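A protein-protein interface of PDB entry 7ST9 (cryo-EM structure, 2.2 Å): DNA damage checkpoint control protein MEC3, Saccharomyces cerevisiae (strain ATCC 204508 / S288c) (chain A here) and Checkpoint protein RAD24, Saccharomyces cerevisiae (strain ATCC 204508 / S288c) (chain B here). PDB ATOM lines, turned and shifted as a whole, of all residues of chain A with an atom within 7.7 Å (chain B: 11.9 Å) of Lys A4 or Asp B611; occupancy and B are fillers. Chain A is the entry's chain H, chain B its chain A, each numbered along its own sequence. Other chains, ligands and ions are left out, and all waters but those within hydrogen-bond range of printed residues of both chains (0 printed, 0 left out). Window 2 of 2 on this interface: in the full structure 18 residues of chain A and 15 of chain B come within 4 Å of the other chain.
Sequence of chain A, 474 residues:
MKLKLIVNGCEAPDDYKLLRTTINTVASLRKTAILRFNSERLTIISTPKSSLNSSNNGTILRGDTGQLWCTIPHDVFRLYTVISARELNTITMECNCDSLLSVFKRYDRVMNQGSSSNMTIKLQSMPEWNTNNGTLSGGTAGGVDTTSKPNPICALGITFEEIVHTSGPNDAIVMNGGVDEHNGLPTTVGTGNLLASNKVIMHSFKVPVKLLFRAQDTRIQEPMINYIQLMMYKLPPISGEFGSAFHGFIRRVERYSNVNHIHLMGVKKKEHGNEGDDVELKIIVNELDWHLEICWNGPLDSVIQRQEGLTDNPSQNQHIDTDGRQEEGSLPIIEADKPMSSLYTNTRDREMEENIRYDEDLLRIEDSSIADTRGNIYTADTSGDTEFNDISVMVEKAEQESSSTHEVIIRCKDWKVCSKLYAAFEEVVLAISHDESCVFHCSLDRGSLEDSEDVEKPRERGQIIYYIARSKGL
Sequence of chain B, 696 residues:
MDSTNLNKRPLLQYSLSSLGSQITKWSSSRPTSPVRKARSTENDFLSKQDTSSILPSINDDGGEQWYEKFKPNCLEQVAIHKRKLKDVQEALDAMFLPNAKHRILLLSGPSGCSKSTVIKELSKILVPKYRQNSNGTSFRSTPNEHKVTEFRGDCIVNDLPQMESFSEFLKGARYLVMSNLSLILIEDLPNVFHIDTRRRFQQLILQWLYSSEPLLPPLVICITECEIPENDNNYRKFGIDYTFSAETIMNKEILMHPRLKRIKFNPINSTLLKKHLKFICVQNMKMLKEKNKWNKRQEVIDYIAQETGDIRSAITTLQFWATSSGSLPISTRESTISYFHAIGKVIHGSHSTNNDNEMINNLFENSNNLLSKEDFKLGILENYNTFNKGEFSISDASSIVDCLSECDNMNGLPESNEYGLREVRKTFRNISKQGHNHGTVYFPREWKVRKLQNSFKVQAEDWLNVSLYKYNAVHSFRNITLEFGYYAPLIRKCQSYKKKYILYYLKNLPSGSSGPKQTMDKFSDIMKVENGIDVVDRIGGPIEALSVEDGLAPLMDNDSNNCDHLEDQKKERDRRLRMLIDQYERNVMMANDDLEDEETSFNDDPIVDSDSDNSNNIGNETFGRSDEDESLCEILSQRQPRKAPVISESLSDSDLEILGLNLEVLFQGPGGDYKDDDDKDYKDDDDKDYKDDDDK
The side-chain carboxylate (OD1) of Asp B611 is in salt-bridge range of the side-chain amino group (NZ) of Lys A4 (3.3 Å). NZ of Lys A2 sits at hydrogen-bond distance from O of Ser B610 (3.4 Å). The side-chain carboxylate (OD1) of Asp B609 lies within salt-bridge range of the side-chain amino group (NZ) of Lys A122.
The backbone carbonyl oxygen of Lys A4 is in hydrogen-bond range of the backbone NH of Thr A81 (3.2 Å).
Lys A4 touches just one residue of chain B: Asp B611. Of chain A, only Lys A4 comes within 4 Å of Asp B611. No residue of chain B comes within 4 Å of Leu A5. Ile A6 touches none of the printed residues of chain B. No residue of chain B comes within 4 Å of Leu A79. No residue of chain B comes within 4 Å of Thr A81. No residue of chain B comes within 4 Å of Ile A121. Lys A122 touches one residue of chain B. Of the printed residues of chain B, Met A1 touches Ile B607 and Val B608. Of the printed residues of chain A, Asp B609 touches Lys A122. The nearest residue of chain A that does not touch Asp B611 is Lys A122 (4.9 Å). The nearest printed residue of chain A that does not touch Asp B609 is Leu A123 (4.1 Å).
Hydrophobic or aromatic side chains of chain A within 4 Å of the printed part of chain B: Met A1 and Leu A123. Along chain A the printed residues that touch a printed residue of chain B span positions 1 to 123. Among the printed residues, Asp or Glu carboxylates within 4 Å of a Lys or Arg side-chain nitrogen of the other chain: Lys A4 with Asp B611 and Lys A122 with Asp B609.
Among the printed residues, pairs that only touch across the chains: Met A1 with Ile B607, Met A1 with Val B608 and Leu A123 with Ile B607.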
ATOM      1  N   MET A   1      23.086  18.096  -1.392  1.00  0.00           N
ATOM      2  CA  MET A   1      22.275  17.781  -0.184  1.00  0.00           C
ATOM      3  C   MET A   1      23.127  17.917   1.078  1.00  0.00           C
ATOM      4  O   MET A   1      23.229  16.980   1.869  1.00  0.00           O
ATOM      5  CB  MET A   1      21.711  16.362  -0.277  1.00  0.00           C
ATOM      6  CG  MET A   1      20.575  16.150  -1.283  1.00  0.00           C
ATOM      7  SD  MET A   1      19.106  17.190  -1.095  1.00  0.00           S
ATOM      8  CE  MET A   1      19.615  18.716  -1.889  1.00  0.00           C
ATOM      9  N   LYS A   2      23.738  19.086   1.263  1.00  0.00           N
ATOM     10  CA  LYS A   2      24.633  19.287   2.396  1.00  0.00           C
ATOM     11  C   LYS A   2      23.879  19.133   3.711  1.00  0.00           C
ATOM     12  O   LYS A   2      22.774  19.658   3.879  1.00  0.00           O
ATOM     13  CB  LYS A   2      25.283  20.669   2.320  1.00  0.00           C
ATOM     14  CG  LYS A   2      26.350  20.907   3.379  1.00  0.00           C
ATOM     15  CD  LYS A   2      27.214  22.113   3.041  1.00  0.00           C
ATOM     16  CE  LYS A   2      28.293  22.341   4.092  1.00  0.00           C
ATOM     17  NZ  LYS A   2      29.276  23.379   3.670  1.00  0.00           N
ATOM     18  N   LEU A   3      24.486  18.407   4.646  1.00  0.00           N
ATOM     19  CA  LEU A   3      23.901  18.159   5.961  1.00  0.00           C
ATOM     20  C   LEU A   3      24.962  18.340   7.044  1.00  0.00           C
ATOM     21  O   LEU A   3      25.111  17.518   7.949  1.00  0.00           O
ATOM     22  CB  LEU A   3      23.283  16.761   6.025  1.00  0.00           C
ATOM     23  CG  LEU A   3      21.897  16.598   5.396  1.00  0.00           C
ATOM     24  CD1 LEU A   3      21.470  15.138   5.425  1.00  0.00           C
ATOM     25  CD2 LEU A   3      20.868  17.471   6.102  1.00  0.00           C
ATOM     26  N   LYS A   4      25.719  19.432   6.956  1.00  0.00           N
ATOM     27  CA  LYS A   4      26.776  19.694   7.925  1.00  0.00           C
ATOM     28  C   LYS A   4      26.166  20.016   9.284  1.00  0.00           C
ATOM     29  O   LYS A   4      25.390  20.968   9.415  1.00  0.00           O
ATOM     30  CB  LYS A   4      27.655  20.845   7.444  1.00  0.00           C
ATOM     31  CG  LYS A   4      28.887  21.086   8.304  1.00  0.00           C
ATOM     32  CD  LYS A   4      29.718  22.243   7.775  1.00  0.00           C
ATOM     33  CE  LYS A   4      31.011  22.404   8.557  1.00  0.00           C
ATOM     34  NZ  LYS A   4      31.872  23.483   7.998  1.00  0.00           N
ATOM     35  N   LEU A   5      26.524  19.227  10.297  1.00  0.00           N
ATOM     36  CA  LEU A   5      26.010  19.389  11.648  1.00  0.00           C
ATOM     37  C   LEU A   5      27.157  19.335  12.646  1.00  0.00           C
ATOM     38  O   LEU A   5      28.147  18.628  12.439  1.00  0.00           O
ATOM     39  CB  LEU A   5      24.980  18.301  11.992  1.00  0.00           C
ATOM     40  CG  LEU A   5      23.696  18.276  11.162  1.00  0.00           C
ATOM     41  CD1 LEU A   5      22.763  17.193  11.671  1.00  0.00           C
ATOM     42  CD2 LEU A   5      23.000  19.626  11.186  1.00  0.00           C
ATOM     43  N   ILE A   6      27.009  20.085  13.736  1.00  0.00           N
ATOM     44  CA  ILE A   6      27.992  20.129  14.811  1.00  0.00           C
ATOM     45  C   ILE A   6      27.288  19.780  16.115  1.00  0.00           C
ATOM     46  O   ILE A   6      26.233  20.342  16.426  1.00  0.00           O
ATOM     47  CB  ILE A   6      28.670  21.510  14.913  1.00  0.00           C
ATOM     48  CG1 ILE A   6      29.471  21.797  13.640  1.00  0.00           C
ATOM     49  CG2 ILE A   6      29.571  21.570  16.142  1.00  0.00           C
ATOM     50  CD1 ILE A   6      30.030  23.203  13.564  1.00  0.00           C
ATOM     51  N   PHE A  77      21.933  21.327  17.804  1.00  0.00           N
ATOM     52  CA  PHE A  77      23.196  21.344  17.083  1.00  0.00           C
ATOM     53  C   PHE A  77      23.755  22.759  17.030  1.00  0.00           C
ATOM     54  O   PHE A  77      23.022  23.724  16.796  1.00  0.00           O
ATOM     55  CB  PHE A  77      23.006  20.802  15.667  1.00  0.00           C
ATOM     56  CG  PHE A  77      22.342  19.456  15.617  1.00  0.00           C
ATOM     57  CD1 PHE A  77      23.077  18.300  15.815  1.00  0.00           C
ATOM     58  CD2 PHE A  77      20.983  19.346  15.375  1.00  0.00           C
ATOM     59  CE1 PHE A  77      22.470  17.058  15.770  1.00  0.00           C
ATOM     60  CE2 PHE A  77      20.370  18.109  15.330  1.00  0.00           C
ATOM     61  CZ  PHE A  77      21.115  16.964  15.528  1.00  0.00           C
ATOM     62  N   ARG A  78      25.066  22.878  17.251  1.00  0.00           N
ATOM     63  CA  ARG A  78      25.705  24.188  17.180  1.00  0.00           C
ATOM     64  C   ARG A  78      25.561  24.788  15.788  1.00  0.00           C
ATOM     65  O   ARG A  78      25.277  25.984  15.645  1.00  0.00           O
ATOM     66  CB  ARG A  78      27.180  24.070  17.567  1.00  0.00           C
ATOM     67  CG  ARG A  78      27.903  25.404  17.684  1.00  0.00           C
ATOM     68  CD  ARG A  78      29.409  25.212  17.767  1.00  0.00           C
ATOM     69  NE  ARG A  78      29.794  24.399  18.915  1.00  0.00           N
ATOM     70  CZ  ARG A  78      29.900  24.854  20.157  1.00  0.00           C
ATOM     71  NH1 ARG A  78      29.651  26.118  20.455  1.00  0.00           N
ATOM     72  NH2 ARG A  78      30.265  24.018  21.125  1.00  0.00           N
ATOM     73  N   LEU A  79      25.753  23.976  14.752  1.00  0.00           N
ATOM     74  CA  LEU A  79      25.582  24.392  13.367  1.00  0.00           C
ATOM     75  C   LEU A  79      24.547  23.491  12.712  1.00  0.00           C
ATOM     76  O   LEU A  79      24.645  22.262  12.799  1.00  0.00           O
ATOM     77  CB  LEU A  79      26.909  24.325  12.605  1.00  0.00           C
ATOM     78  CG  LEU A  79      26.849  24.608  11.102  1.00  0.00           C
ATOM     79  CD1 LEU A  79      26.304  26.003  10.836  1.00  0.00           C
ATOM     80  CD2 LEU A  79      28.224  24.439  10.474  1.00  0.00           C
ATOM     81  N   TYR A  80      23.557  24.101  12.060  1.00  0.00           N
ATOM     82  CA  TYR A  80      22.478  23.375  11.389  1.00  0.00           C
ATOM     83  C   TYR A  80      22.425  23.865   9.945  1.00  0.00           C
ATOM     84  O   TYR A  80      21.680  24.793   9.622  1.00  0.00           O
ATOM     85  CB  TYR A  80      21.145  23.582  12.107  1.00  0.00           C
ATOM     86  CG  TYR A  80      20.091  22.559  11.748  1.00  0.00           C
ATOM     87  CD1 TYR A  80      20.279  21.212  12.029  1.00  0.00           C
ATOM     88  CD2 TYR A  80      18.909  22.938  11.125  1.00  0.00           C
ATOM     89  CE1 TYR A  80      19.321  20.273  11.705  1.00  0.00           C
ATOM     90  CE2 TYR A  80      17.944  22.004  10.797  1.00  0.00           C
ATOM     91  CZ  TYR A  80      18.156  20.673  11.089  1.00  0.00           C
ATOM     92  OH  TYR A  80      17.201  19.738  10.765  1.00  0.00           O
ATOM     93  N   THR A  81      23.217  23.238   9.081  1.00  0.00           N
ATOM     94  CA  THR A  81      23.280  23.575   7.661  1.00  0.00           C
ATOM     95  C   THR A  81      22.545  22.477   6.896  1.00  0.00           C
ATOM     96  O   THR A  81      23.146  21.494   6.458  1.00  0.00           O
ATOM     97  CB  THR A  81      24.727  23.714   7.189  1.00  0.00           C
ATOM     98  OG1 THR A  81      25.409  24.677   8.003  1.00  0.00           O
ATOM     99  CG2 THR A  81      24.775  24.158   5.733  1.00  0.00           C
ATOM    100  N   VAL A  82      21.236  22.652   6.739  1.00  0.00           N
ATOM    101  CA  VAL A  82      20.384  21.702   6.034  1.00  0.00           C
ATOM    102  C   VAL A  82      19.752  22.455   4.871  1.00  0.00           C
ATOM    103  O   VAL A  82      18.810  23.235   5.061  1.00  0.00           O
ATOM    104  CB  VAL A  82      19.318  21.088   6.948  1.00  0.00           C
ATOM    105  CG1 VAL A  82      18.411  20.154   6.158  1.00  0.00           C
ATOM    106  CG2 VAL A  82      19.975  20.349   8.103  1.00  0.00           C
ATOM    107  N   ILE A  83      20.266  22.228   3.666  1.00  0.00           N
ATOM    108  CA  ILE A  83      19.755  22.848   2.450  1.00  0.00           C
ATOM    109  C   ILE A  83      19.297  21.740   1.514  1.00  0.00           C
ATOM    110  O   ILE A  83      20.060  20.811   1.224  1.00  0.00           O
ATOM    111  CB  ILE A  83      20.815  23.735   1.768  1.00  0.00           C
ATOM    112  CG1 ILE A  83      21.493  24.650   2.791  1.00  0.00           C
ATOM    113  CG2 ILE A  83      20.176  24.566   0.664  1.00  0.00           C
ATOM    114  CD1 ILE A  83      22.661  25.434   2.230  1.00  0.00           C
ATOM    115  N   MET A 119      31.749  17.159  17.562  1.00  0.00           N
ATOM    116  CA  MET A 119      31.539  16.118  16.564  1.00  0.00           C
ATOM    117  C   MET A 119      30.933  16.749  15.317  1.00  0.00           C
ATOM    118  O   MET A 119      29.878  17.389  15.392  1.00  0.00           O
ATOM    119  CB  MET A 119      30.630  15.018  17.113  1.00  0.00           C
ATOM    120  CG  MET A 119      29.808  14.292  16.052  1.00  0.00           C
ATOM    121  SD  MET A 119      29.107  12.727  16.619  1.00  0.00           S
ATOM    122  CE  MET A 119      30.575  11.830  17.122  1.00  0.00           C
ATOM    123  N   THR A 120      31.596  16.568  14.179  1.00  0.00           N
ATOM    124  CA  THR A 120      31.140  17.096  12.901  1.00  0.00           C
ATOM    125  C   THR A 120      30.577  15.958  12.063  1.00  0.00           C
ATOM    126  O   THR A 120      31.250  14.942  11.859  1.00  0.00           O
ATOM    127  CB  THR A 120      32.282  17.789  12.153  1.00  0.00           C
ATOM    128  OG1 THR A 120      32.849  18.813  12.979  1.00  0.00           O
ATOM    129  CG2 THR A 120      31.777  18.408  10.856  1.00  0.00           C
ATOM    130  N   ILE A 121      29.348  16.135  11.579  1.00  0.00           N
ATOM    131  CA  ILE A 121      28.647  15.133  10.787  1.00  0.00           C
ATOM    132  C   ILE A 121      28.338  15.726   9.420  1.00  0.00           C
ATOM    133  O   ILE A 121      27.905  16.879   9.316  1.00  0.00           O
ATOM    134  CB  ILE A 121      27.351  14.660  11.480  1.00  0.00           C
ATOM    135  CG1 ILE A 121      27.664  14.072  12.858  1.00  0.00           C
ATOM    136  CG2 ILE A 121      26.631  13.631  10.621  1.00  0.00           C
ATOM    137  CD1 ILE A 121      26.857  14.691  13.979  1.00  0.00           C
ATOM    138  N   LYS A 122      28.564  14.935   8.373  1.00  0.00           N
ATOM    139  CA  LYS A 122      28.331  15.385   7.009  1.00  0.00           C
ATOM    140  C   LYS A 122      27.879  14.204   6.162  1.00  0.00           C
ATOM    141  O   LYS A 122      28.094  13.043   6.517  1.00  0.00           O
ATOM    142  CB  LYS A 122      29.588  16.020   6.403  1.00  0.00           C
ATOM    143  CG  LYS A 122      29.998  17.331   7.054  1.00  0.00           C
ATOM    144  CD  LYS A 122      31.096  18.026   6.265  1.00  0.00           C
ATOM    145  CE  LYS A 122      32.408  17.262   6.339  1.00  0.00           C
ATOM    146  NZ  LYS A 122      33.516  17.984   5.656  1.00  0.00           N
ATOM    147  N   LEU A 123      27.244  14.516   5.037  1.00  0.00           N
ATOM    148  CA  LEU A 123      26.800  13.514   4.076  1.00  0.00           C
ATOM    149  C   LEU A 123      27.791  13.478   2.920  1.00  0.00           C
ATOM    150  O   LEU A 123      28.052  14.508   2.290  1.00  0.00           O
ATOM    151  CB  LEU A 123      25.391  13.831   3.573  1.00  0.00           C
ATOM    152  CG  LEU A 123      24.689  12.733   2.773  1.00  0.00           C
ATOM    153  CD1 LEU A 123      24.381  11.530   3.652  1.00  0.00           C
ATOM    154  CD2 LEU A 123      23.417  13.271   2.136  1.00  0.00           C
ATOM    155  N   ILE B 607      24.500  15.280  -4.085  1.00  0.00           N
ATOM    156  CA  ILE B 607      25.175  15.666  -2.850  1.00  0.00           C
ATOM    157  C   ILE B 607      26.338  16.589  -3.185  1.00  0.00           C
ATOM    158  O   ILE B 607      26.978  16.445  -4.232  1.00  0.00           O
ATOM    159  CB  ILE B 607      25.671  14.438  -2.058  1.00  0.00           C
ATOM    160  CG1 ILE B 607      26.408  13.441  -2.964  1.00  0.00           C
ATOM    161  CG2 ILE B 607      24.506  13.752  -1.362  1.00  0.00           C
ATOM    162  CD1 ILE B 607      27.906  13.646  -3.001  1.00  0.00           C
ATOM    163  N   VAL B 608      26.613  17.547  -2.302  1.00  0.00           N
ATOM    164  CA  VAL B 608      27.755  18.443  -2.434  1.00  0.00           C
ATOM    165  C   VAL B 608      28.512  18.424  -1.115  1.00  0.00           C
ATOM    166  O   VAL B 608      27.955  18.784  -0.071  1.00  0.00           O
ATOM    167  CB  VAL B 608      27.329  19.876  -2.796  1.00  0.00           C
ATOM    168  CG1 VAL B 608      28.551  20.774  -2.936  1.00  0.00           C
ATOM    169  CG2 VAL B 608      26.508  19.878  -4.076  1.00  0.00           C
ATOM    170  N   ASP B 609      29.776  18.007  -1.159  1.00  0.00           N
ATOM    171  CA  ASP B 609      30.628  17.926   0.020  1.00  0.00           C
ATOM    172  C   ASP B 609      31.846  18.809  -0.196  1.00  0.00           C
ATOM    173  O   ASP B 609      32.640  18.565  -1.112  1.00  0.00           O
ATOM    174  CB  ASP B 609      31.050  16.480   0.294  1.00  0.00           C
ATOM    175  CG  ASP B 609      31.922  16.350   1.527  1.00  0.00           C
ATOM    176  OD1 ASP B 609      31.683  17.087   2.506  1.00  0.00           O
ATOM    177  OD2 ASP B 609      32.846  15.510   1.517  1.00  0.00           O
ATOM    178  N   SER B 610      31.993  19.831   0.644  1.00  0.00           N
ATOM    179  CA  SER B 610      33.121  20.748   0.553  1.00  0.00           C
ATOM    180  C   SER B 610      33.123  21.637   1.786  1.00  0.00           C
ATOM    181  O   SER B 610      32.064  21.972   2.325  1.00  0.00           O
ATOM    182  CB  SER B 610      33.053  21.599  -0.720  1.00  0.00           C
ATOM    183  OG  SER B 610      34.192  22.433  -0.838  1.00  0.00           O
ATOM    184  N   ASP B 611      34.321  22.013   2.222  1.00  0.00           N
ATOM    185  CA  ASP B 611      34.479  22.874   3.389  1.00  0.00           C
ATOM    186  C   ASP B 611      34.905  24.276   2.971  1.00  0.00           C
ATOM    187  O   ASP B 611      35.774  24.442   2.115  1.00  0.00           O
ATOM    188  CB  ASP B 611      35.503  22.279   4.358  1.00  0.00           C
ATOM    189  CG  ASP B 611      35.476  22.949   5.718  1.00  0.00           C
ATOM    190  OD1 ASP B 611      34.518  23.701   5.995  1.00  0.00           O
ATOM    191  OD2 ASP B 611      36.412  22.722   6.513  1.00  0.00           O
